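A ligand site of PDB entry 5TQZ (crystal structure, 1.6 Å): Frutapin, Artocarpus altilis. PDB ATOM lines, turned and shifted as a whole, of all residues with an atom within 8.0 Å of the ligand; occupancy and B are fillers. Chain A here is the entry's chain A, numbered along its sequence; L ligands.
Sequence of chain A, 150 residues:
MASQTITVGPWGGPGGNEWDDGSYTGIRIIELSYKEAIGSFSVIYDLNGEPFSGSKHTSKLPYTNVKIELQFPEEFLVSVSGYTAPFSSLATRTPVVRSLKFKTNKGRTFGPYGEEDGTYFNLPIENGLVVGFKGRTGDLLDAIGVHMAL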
ATOM      1  N   GLY A  13      -4.459  -3.915  26.216  1.00  0.00           N
ATOM      2  CA  GLY A  13      -5.210  -3.361  27.275  1.00  0.00           C
ATOM      3  C   GLY A  13      -6.485  -4.081  27.517  1.00  0.00           C
ATOM      4  O   GLY A  13      -6.793  -5.069  26.838  1.00  0.00           O
ATOM      5  N   PRO A  14      -7.236  -3.704  28.537  1.00  0.00           N
ATOM      6  CA  PRO A  14      -8.446  -4.520  29.059  1.00  0.00           C
ATOM      7  C   PRO A  14      -9.738  -4.199  28.328  1.00  0.00           C
ATOM      8  O   PRO A  14     -10.823  -4.727  28.571  1.00  0.00           O
ATOM      9  CB  PRO A  14      -8.401  -4.175  30.564  1.00  0.00           C
ATOM     10  CG  PRO A  14      -8.072  -2.762  30.485  1.00  0.00           C
ATOM     11  CD  PRO A  14      -6.966  -2.580  29.474  1.00  0.00           C
ATOM     12  N   GLY A  15      -9.695  -3.409  27.249  1.00  0.00           N
ATOM     13  CA  GLY A  15     -10.972  -3.079  26.515  1.00  0.00           C
ATOM     14  C   GLY A  15     -11.482  -4.198  25.565  1.00  0.00           C
ATOM     15  O   GLY A  15     -10.736  -5.196  25.293  1.00  0.00           O
ATOM     16  N   GLY A  16     -12.618  -3.912  24.943  1.00  0.00           N
ATOM     17  CA  GLY A  16     -13.286  -4.792  23.980  1.00  0.00           C
ATOM     18  C   GLY A  16     -13.722  -6.072  24.733  1.00  0.00           C
ATOM     19  O   GLY A  16     -13.759  -6.082  25.899  1.00  0.00           O
ATOM     20  N   ASN A  17     -14.004  -7.112  23.983  1.00  0.00           N
ATOM     21  CA  ASN A  17     -14.345  -8.464  24.569  1.00  0.00           C
ATOM     22  C   ASN A  17     -13.246  -9.493  24.272  1.00  0.00           C
ATOM     23  O   ASN A  17     -12.656  -9.578  23.177  1.00  0.00           O
ATOM     24  CB  ASN A  17     -15.670  -8.947  24.026  1.00  0.00           C
ATOM     25  CG  ASN A  17     -16.763  -7.876  24.080  1.00  0.00           C
ATOM     26  OD1 ASN A  17     -16.893  -7.237  25.074  1.00  0.00           O
ATOM     27  ND2 ASN A  17     -17.551  -7.754  23.080  1.00  0.00           N
ATOM     28  N   ILE A  38      -4.231  -1.904  14.735  1.00  0.00           N
ATOM     29  CA  ILE A  38      -4.782  -3.198  14.241  1.00  0.00           C
ATOM     30  C   ILE A  38      -6.322  -3.314  14.458  1.00  0.00           C
ATOM     31  O   ILE A  38      -6.802  -3.128  15.575  1.00  0.00           O
ATOM     32  CB  ILE A  38      -4.045  -4.365  14.837  1.00  0.00           C
ATOM     33  CG1 ILE A  38      -2.516  -4.325  14.564  1.00  0.00           C
ATOM     34  CG2 ILE A  38      -4.583  -5.666  14.291  1.00  0.00           C
ATOM     35  CD1 ILE A  38      -2.130  -4.330  13.091  1.00  0.00           C
ATOM     36  N   GLY A  39      -7.045  -3.595  13.373  1.00  0.00           N
ATOM     37  CA  GLY A  39      -8.462  -3.828  13.402  1.00  0.00           C
ATOM     38  C   GLY A  39      -8.822  -5.348  13.569  1.00  0.00           C
ATOM     39  O   GLY A  39      -8.862  -5.935  14.735  1.00  0.00           O
ATOM     40  N   SER A  59     -12.964  -6.379  12.585  1.00  0.00           N
ATOM     41  CA  SER A  59     -13.377  -4.938  12.723  1.00  0.00           C
ATOM     42  C   SER A  59     -14.152  -4.468  11.513  1.00  0.00           C
ATOM     43  O   SER A  59     -13.702  -4.694  10.369  1.00  0.00           O
ATOM     44  CB  SER A  59     -12.148  -3.982  12.889  1.00  0.00           C
ATOM     45  OG  SER A  59     -12.570  -2.626  12.987  1.00  0.00           O
ATOM     46  N   LYS A  60     -15.297  -3.822  11.777  1.00  0.00           N
ATOM     47  CA  LYS A  60     -16.040  -3.039  10.753  1.00  0.00           C
ATOM     48  C   LYS A  60     -15.397  -1.704  10.228  1.00  0.00           C
ATOM     49  O   LYS A  60     -15.813  -1.148   9.224  1.00  0.00           O
ATOM     50  CB  LYS A  60     -17.524  -2.813  11.093  1.00  0.00           C
ATOM     51  CG  LYS A  60     -17.848  -2.048  12.371  1.00  0.00           C
ATOM     52  CD  LYS A  60     -19.380  -1.919  12.519  1.00  0.00           C
ATOM     53  CE  LYS A  60     -19.918  -0.481  12.692  1.00  0.00           C
ATOM     54  NZ  LYS A  60     -19.821  -0.030  14.114  1.00  0.00           N
ATOM     55  N   LEU A  61     -14.389  -1.219  10.916  1.00  0.00           N
ATOM     56  CA  LEU A  61     -13.650  -0.045  10.405  1.00  0.00           C
ATOM     57  C   LEU A  61     -13.097  -0.293   9.002  1.00  0.00           C
ATOM     58  O   LEU A  61     -12.601  -1.360   8.763  1.00  0.00           O
ATOM     59  CB  LEU A  61     -12.459   0.347  11.333  1.00  0.00           C
ATOM     60  CG  LEU A  61     -12.853   0.626  12.808  1.00  0.00           C
ATOM     61  CD1 LEU A  61     -11.600   1.166  13.588  1.00  0.00           C
ATOM     62  CD2 LEU A  61     -13.994   1.625  12.892  1.00  0.00           C
ATOM     63  N   PHE A  87      -5.608   4.793  21.318  1.00  0.00           N
ATOM     64  CA  PHE A  87      -5.842   5.434  20.004  1.00  0.00           C
ATOM     65  C   PHE A  87      -7.072   6.307  20.136  1.00  0.00           C
ATOM     66  O   PHE A  87      -8.233   5.830  20.062  1.00  0.00           O
ATOM     67  CB  PHE A  87      -5.863   4.392  18.881  1.00  0.00           C
ATOM     68  CG  PHE A  87      -6.242   4.987  17.558  1.00  0.00           C
ATOM     69  CD1 PHE A  87      -5.445   5.996  16.997  1.00  0.00           C
ATOM     70  CD2 PHE A  87      -7.375   4.569  16.890  1.00  0.00           C
ATOM     71  CE1 PHE A  87      -5.812   6.623  15.777  1.00  0.00           C
ATOM     72  CE2 PHE A  87      -7.767   5.210  15.687  1.00  0.00           C
ATOM     73  CZ  PHE A  87      -6.990   6.213  15.137  1.00  0.00           C
ATOM     74  N   SER A  89      -9.380   8.396  19.854  1.00  0.00           N
ATOM     75  CA  SER A  89     -10.876   8.462  19.765  1.00  0.00           C
ATOM     76  C   SER A  89     -11.709   7.224  20.333  1.00  0.00           C
ATOM     77  O   SER A  89     -12.402   7.294  21.381  1.00  0.00           O
ATOM     78  CB  SER A  89     -11.285   8.742  18.320  1.00  0.00           C
ATOM     79  OG  SER A  89     -12.689   8.947  18.296  1.00  0.00           O
ATOM     80  N   LEU A  90     -11.632   6.083  19.665  1.00  0.00           N
ATOM     81  CA  LEU A  90     -12.405   4.914  20.187  1.00  0.00           C
ATOM     82  C   LEU A  90     -11.750   4.170  21.365  1.00  0.00           C
ATOM     83  O   LEU A  90     -12.423   3.344  21.967  1.00  0.00           O
ATOM     84  CB  LEU A  90     -12.815   3.880  19.105  1.00  0.00           C
ATOM     85  CG  LEU A  90     -12.298   3.914  17.657  1.00  0.00           C
ATOM     86  CD1 LEU A  90     -10.785   3.939  17.677  1.00  0.00           C
ATOM     87  CD2 LEU A  90     -12.770   2.664  16.923  1.00  0.00           C
ATOM     88  N   ALA A  91     -10.451   4.412  21.649  1.00  0.00           N
ATOM     89  CA  ALA A  91      -9.741   3.781  22.807  1.00  0.00           C
ATOM     90  C   ALA A  91      -8.937   4.846  23.406  1.00  0.00           C
ATOM     91  O   ALA A  91      -7.659   4.924  23.306  1.00  0.00           O
ATOM     92  CB  ALA A  91      -8.860   2.669  22.380  1.00  0.00           C
ATOM     93  N   THR A  92      -9.686   5.670  24.099  1.00  0.00           N
ATOM     94  CA  THR A  92      -9.081   6.881  24.887  1.00  0.00           C
ATOM     95  C   THR A  92      -8.508   6.489  26.223  1.00  0.00           C
ATOM     96  O   THR A  92      -7.615   7.207  26.806  1.00  0.00           O
ATOM     97  CB  THR A  92     -10.189   7.946  25.133  1.00  0.00           C
ATOM     98  OG1 THR A  92     -10.818   8.128  23.848  1.00  0.00           O
ATOM     99  CG2 THR A  92      -9.675   9.260  25.508  1.00  0.00           C
ATOM    100  N   ARG A  93      -9.058   5.381  26.783  1.00  0.00           N
ATOM    101  CA  ARG A  93      -8.730   5.033  28.183  1.00  0.00           C
ATOM    102  C   ARG A  93      -7.812   3.921  28.297  1.00  0.00           C
ATOM    103  O   ARG A  93      -7.242   3.839  29.344  1.00  0.00           O
ATOM    104  CB  ARG A  93     -10.011   4.702  28.970  1.00  0.00           C
ATOM    105  CG  ARG A  93     -10.959   5.758  28.945  1.00  0.00           C
ATOM    106  CD  ARG A  93     -12.189   5.297  29.795  1.00  0.00           C
ATOM    107  NE  ARG A  93     -12.880   6.405  30.198  1.00  0.00           N
ATOM    108  CZ  ARG A  93     -12.838   6.949  31.411  1.00  0.00           C
ATOM    109  NH1 ARG A  93     -12.162   6.293  32.411  1.00  0.00           N
ATOM    110  NH2 ARG A  93     -13.603   7.903  31.641  1.00  0.00           N
ATOM    111  N   THR A  94      -7.650   2.992  27.285  1.00  0.00           N
ATOM    112  CA  THR A  94      -6.964   1.801  27.459  1.00  0.00           C
ATOM    113  C   THR A  94      -6.122   1.568  26.202  1.00  0.00           C
ATOM    114  O   THR A  94      -6.537   2.003  25.110  1.00  0.00           O
ATOM    115  CB  THR A  94      -7.948   0.586  27.812  1.00  0.00           C
ATOM    116  OG1 THR A  94      -9.033   0.404  26.882  1.00  0.00           O
ATOM    117  CG2 THR A  94      -8.522   0.937  29.128  1.00  0.00           C
ATOM    118  N   PRO A  95      -4.909   1.015  26.356  1.00  0.00           N
ATOM    119  CA  PRO A  95      -4.113   0.689  25.209  1.00  0.00           C
ATOM    120  C   PRO A  95      -4.642  -0.412  24.304  1.00  0.00           C
ATOM    121  O   PRO A  95      -5.369  -1.209  24.761  1.00  0.00           O
ATOM    122  CB  PRO A  95      -2.716   0.288  25.794  1.00  0.00           C
ATOM    123  CG  PRO A  95      -3.032  -0.136  27.140  1.00  0.00           C
ATOM    124  CD  PRO A  95      -4.320   0.501  27.615  1.00  0.00           C
ATOM    125  N   VAL A  96      -4.473  -0.264  22.981  1.00  0.00           N
ATOM    126  CA  VAL A  96      -4.801  -1.285  22.006  1.00  0.00           C
ATOM    127  C   VAL A  96      -3.572  -1.705  21.331  1.00  0.00           C
ATOM    128  O   VAL A  96      -2.553  -1.071  21.571  1.00  0.00           O
ATOM    129  CB  VAL A  96      -5.786  -0.795  21.015  1.00  0.00           C
ATOM    130  CG1 VAL A  96      -7.047  -0.271  21.770  1.00  0.00           C
ATOM    131  CG2 VAL A  96      -5.240   0.268  20.071  1.00  0.00           C
ATOM    132  N   VAL A  97      -3.641  -2.669  20.395  1.00  0.00           N
ATOM    133  CA  VAL A  97      -2.403  -3.081  19.625  1.00  0.00           C
ATOM    134  C   VAL A  97      -2.414  -2.122  18.473  1.00  0.00           C
ATOM    135  O   VAL A  97      -3.384  -2.151  17.646  1.00  0.00           O
ATOM    136  CB  VAL A  97      -2.570  -4.546  19.245  1.00  0.00           C
ATOM    137  CG1 VAL A  97      -1.376  -4.978  18.346  1.00  0.00           C
ATOM    138  CG2 VAL A  97      -2.801  -5.416  20.492  1.00  0.00           C
ATOM    139  N   ARG A 136      -8.132  -9.753  22.637  1.00  0.00           N
ATOM    140  CA  ARG A 136      -9.411  -9.044  22.967  1.00  0.00           C
ATOM    141  C   ARG A 136      -9.661  -8.135  21.851  1.00  0.00           C
ATOM    142  O   ARG A 136      -8.697  -7.424  21.408  1.00  0.00           O
ATOM    143  CB  ARG A 136      -9.231  -8.168  24.289  1.00  0.00           C
ATOM    144  CG  ARG A 136      -8.868  -8.980  25.644  1.00  0.00           C
ATOM    145  CD  ARG A 136      -8.804  -8.001  26.874  1.00  0.00           C
ATOM    146  NE  ARG A 136     -10.097  -7.394  27.101  1.00  0.00           N
ATOM    147  CZ  ARG A 136     -11.060  -8.014  27.801  1.00  0.00           C
ATOM    148  NH1 ARG A 136     -10.912  -9.244  28.419  1.00  0.00           N
ATOM    149  NH2 ARG A 136     -12.270  -7.549  27.842  1.00  0.00           N
ATOM    150  N   THR A 137     -10.931  -8.029  21.455  1.00  0.00           N
ATOM    151  CA  THR A 137     -11.301  -7.241  20.313  1.00  0.00           C
ATOM    152  C   THR A 137     -12.538  -6.440  20.605  1.00  0.00           C
ATOM    153  O   THR A 137     -13.551  -7.040  21.002  1.00  0.00           O
ATOM    154  CB  THR A 137     -11.523  -8.037  19.032  1.00  0.00           C
ATOM    155  OG1 THR A 137     -10.332  -8.803  18.737  1.00  0.00           O
ATOM    156  CG2 THR A 137     -11.989  -7.120  17.857  1.00  0.00           C
ATOM    157  N   GLY A 138     -12.535  -5.185  20.256  1.00  0.00           N
ATOM    158  CA  GLY A 138     -13.751  -4.358  20.182  1.00  0.00           C
ATOM    159  C   GLY A 138     -14.019  -3.834  18.791  1.00  0.00           C
ATOM    160  O   GLY A 138     -14.446  -4.564  17.961  1.00  0.00           O
ATOM    161  N   ASP A 139     -13.870  -2.530  18.564  1.00  0.00           N
ATOM    162  CA  ASP A 139     -13.665  -2.080  17.169  1.00  0.00           C
ATOM    163  C   ASP A 139     -12.331  -2.310  16.746  1.00  0.00           C
ATOM    164  O   ASP A 139     -12.043  -2.271  15.544  1.00  0.00           O
ATOM    165  CB  ASP A 139     -13.958  -0.601  17.061  1.00  0.00           C
ATOM    166  CG  ASP A 139     -15.420  -0.333  17.083  1.00  0.00           C
ATOM    167  OD1 ASP A 139     -16.084  -0.978  16.226  1.00  0.00           O
ATOM    168  OD2 ASP A 139     -15.884   0.434  17.995  1.00  0.00           O
ATOM    169  N   LEU A 140     -11.442  -2.573  17.673  1.00  0.00           N
ATOM    170  CA  LEU A 140      -9.991  -2.724  17.432  1.00  0.00           C
ATOM    171  C   LEU A 140      -9.500  -3.957  18.174  1.00  0.00           C
ATOM    172  O   LEU A 140     -10.187  -4.546  19.057  1.00  0.00           O
ATOM    173  CB  LEU A 140      -9.125  -1.509  17.984  1.00  0.00           C
ATOM    174  CG  LEU A 140      -9.379  -0.260  17.172  1.00  0.00           C
ATOM    175  CD1 LEU A 140      -8.883   0.849  17.939  1.00  0.00           C
ATOM    176  CD2 LEU A 140      -8.739  -0.158  15.814  1.00  0.00           C
ATOM    177  N   LEU A 141      -8.311  -4.359  17.792  1.00  0.00           N
ATOM    178  CA  LEU A 141      -7.514  -5.445  18.528  1.00  0.00           C
ATOM    179  C   LEU A 141      -6.995  -4.827  19.786  1.00  0.00           C
ATOM    180  O   LEU A 141      -5.930  -4.163  19.727  1.00  0.00           O
ATOM    181  CB  LEU A 141      -6.406  -6.021  17.709  1.00  0.00           C
ATOM    182  CG  LEU A 141      -5.674  -7.241  18.361  1.00  0.00           C
ATOM    183  CD1 LEU A 141      -6.618  -8.464  18.607  1.00  0.00           C
ATOM    184  CD2 LEU A 141      -4.397  -7.682  17.637  1.00  0.00           C
ATOM    185  N   ASP A 142      -7.732  -4.906  20.906  1.00  0.00           N
ATOM    186  CA  ASP A 142      -7.292  -4.364  22.134  1.00  0.00           C
ATOM    187  C   ASP A 142      -6.030  -5.048  22.690  1.00  0.00           C
ATOM    188  O   ASP A 142      -5.117  -4.355  23.329  1.00  0.00           O
ATOM    189  CB  ASP A 142      -8.396  -4.437  23.212  1.00  0.00           C
ATOM    190  CG  ASP A 142      -9.468  -3.457  22.949  1.00  0.00           C
ATOM    191  OD1 ASP A 142     -10.229  -3.811  22.063  1.00  0.00           O
ATOM    192  OD2 ASP A 142      -9.418  -2.373  23.508  1.00  0.00           O
ATOM    193  N   ALA A 143      -6.021  -6.409  22.580  1.00  0.00           N
ATOM    194  CA  ALA A 143      -4.951  -7.201  23.242  1.00  0.00           C
ATOM    195  C   ALA A 143      -4.598  -8.422  22.415  1.00  0.00           C
ATOM    196  O   ALA A 143      -5.506  -8.890  21.709  1.00  0.00           O
ATOM    197  CB  ALA A 143      -5.355  -7.638  24.640  1.00  0.00           C
HETATM  198  C1  LIG L   1     -14.730  -0.812  21.317  1.00  0.00           C
HETATM  199  C2  LIG L   1     -14.967  -0.930  22.835  1.00  0.00           C
HETATM  200  C3  LIG L   1     -13.716  -0.603  23.694  1.00  0.00           C
HETATM  201  C4  LIG L   1     -12.431  -1.031  23.011  1.00  0.00           C
HETATM  202  C5  LIG L   1     -12.345  -0.206  21.756  1.00  0.00           C
HETATM  203  C6  LIG L   1     -11.357  -0.659  20.749  1.00  0.00           C
HETATM  204  O1  LIG L   1     -15.652  -0.279  20.325  1.00  0.00           O
HETATM  205  O2  LIG L   1     -16.096  -0.262  23.382  1.00  0.00           O
HETATM  206  O3  LIG L   1     -13.856  -1.313  24.925  1.00  0.00           O
HETATM  207  O4  LIG L   1     -11.320  -0.710  23.858  1.00  0.00           O
HETATM  208  O5  LIG L   1     -13.561  -0.084  21.033  1.00  0.00           O
HETATM  209  O6  LIG L   1     -11.486  -2.065  20.472  1.00  0.00           O
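An oxygen (O6) of the ligand is in hydrogen-bond range of the backbone NH (N) of Asp 139. The side-chain carboxylate of Asp 139 is in hydrogen-bond range of an oxygen (O1) of the ligand. The side-chain carboxylate (OD2) of Asp 142 sits at hydrogen-bond distance from an oxygen (O4) of the ligand (2.6 Å). The backbone NH (N) of Leu 140 is in hydrogen-bond range of an oxygen (O6) of the ligand, at 2.8 Å. O of Leu 140 is in hydrogen-bond range of O6 of the ligand (3.1 Å). The backbone NH (N) of Gly 16 is in hydrogen-bond range of an oxygen (O3) of the ligand (2.9 Å). The backbone NH of Gly 138 lies close to an oxygen (O6) of the ligand (3.3 Å).
OG of Ser 59 is in hydrogen-bond range of O of Asp 139 (2.6 Å). N of Gly 138 lies within hydrogen-bond range of OD1 of Asp 142, at 3.2 Å. The backbone carbonyl oxygen (O) of Arg 136 is in hydrogen-bond range of the backbone NH (N) of Asp 142, 2.7 Å away. O of Asp 142 is in hydrogen-bond range of N of Gly 13 (3.0 Å). The backbone carbonyl oxygen of Gly 16 sits at hydrogen-bond distance from the guanidinium group of Arg 136 (2.9 Å). The guanidinium group of Arg 136 sits at hydrogen-bond distance from the backbone carbonyl oxygen of Gly 15, at 2.9 Å.
Gly 15 touches the ligand. O of Leu 90 touches C5 of the ligand (3.6 Å). Thr 94 touches the ligand (OG1 to O4, 3.95 Å). Hydrophobic or aromatic side chains within 4 Å of the ligand: Leu 140. Eight residues have an atom within 4 Å of the ligand: Gly 15, Gly 16, Leu 90, Thr 94, Gly 138, Asp 139, Leu 140 and Asp 142.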
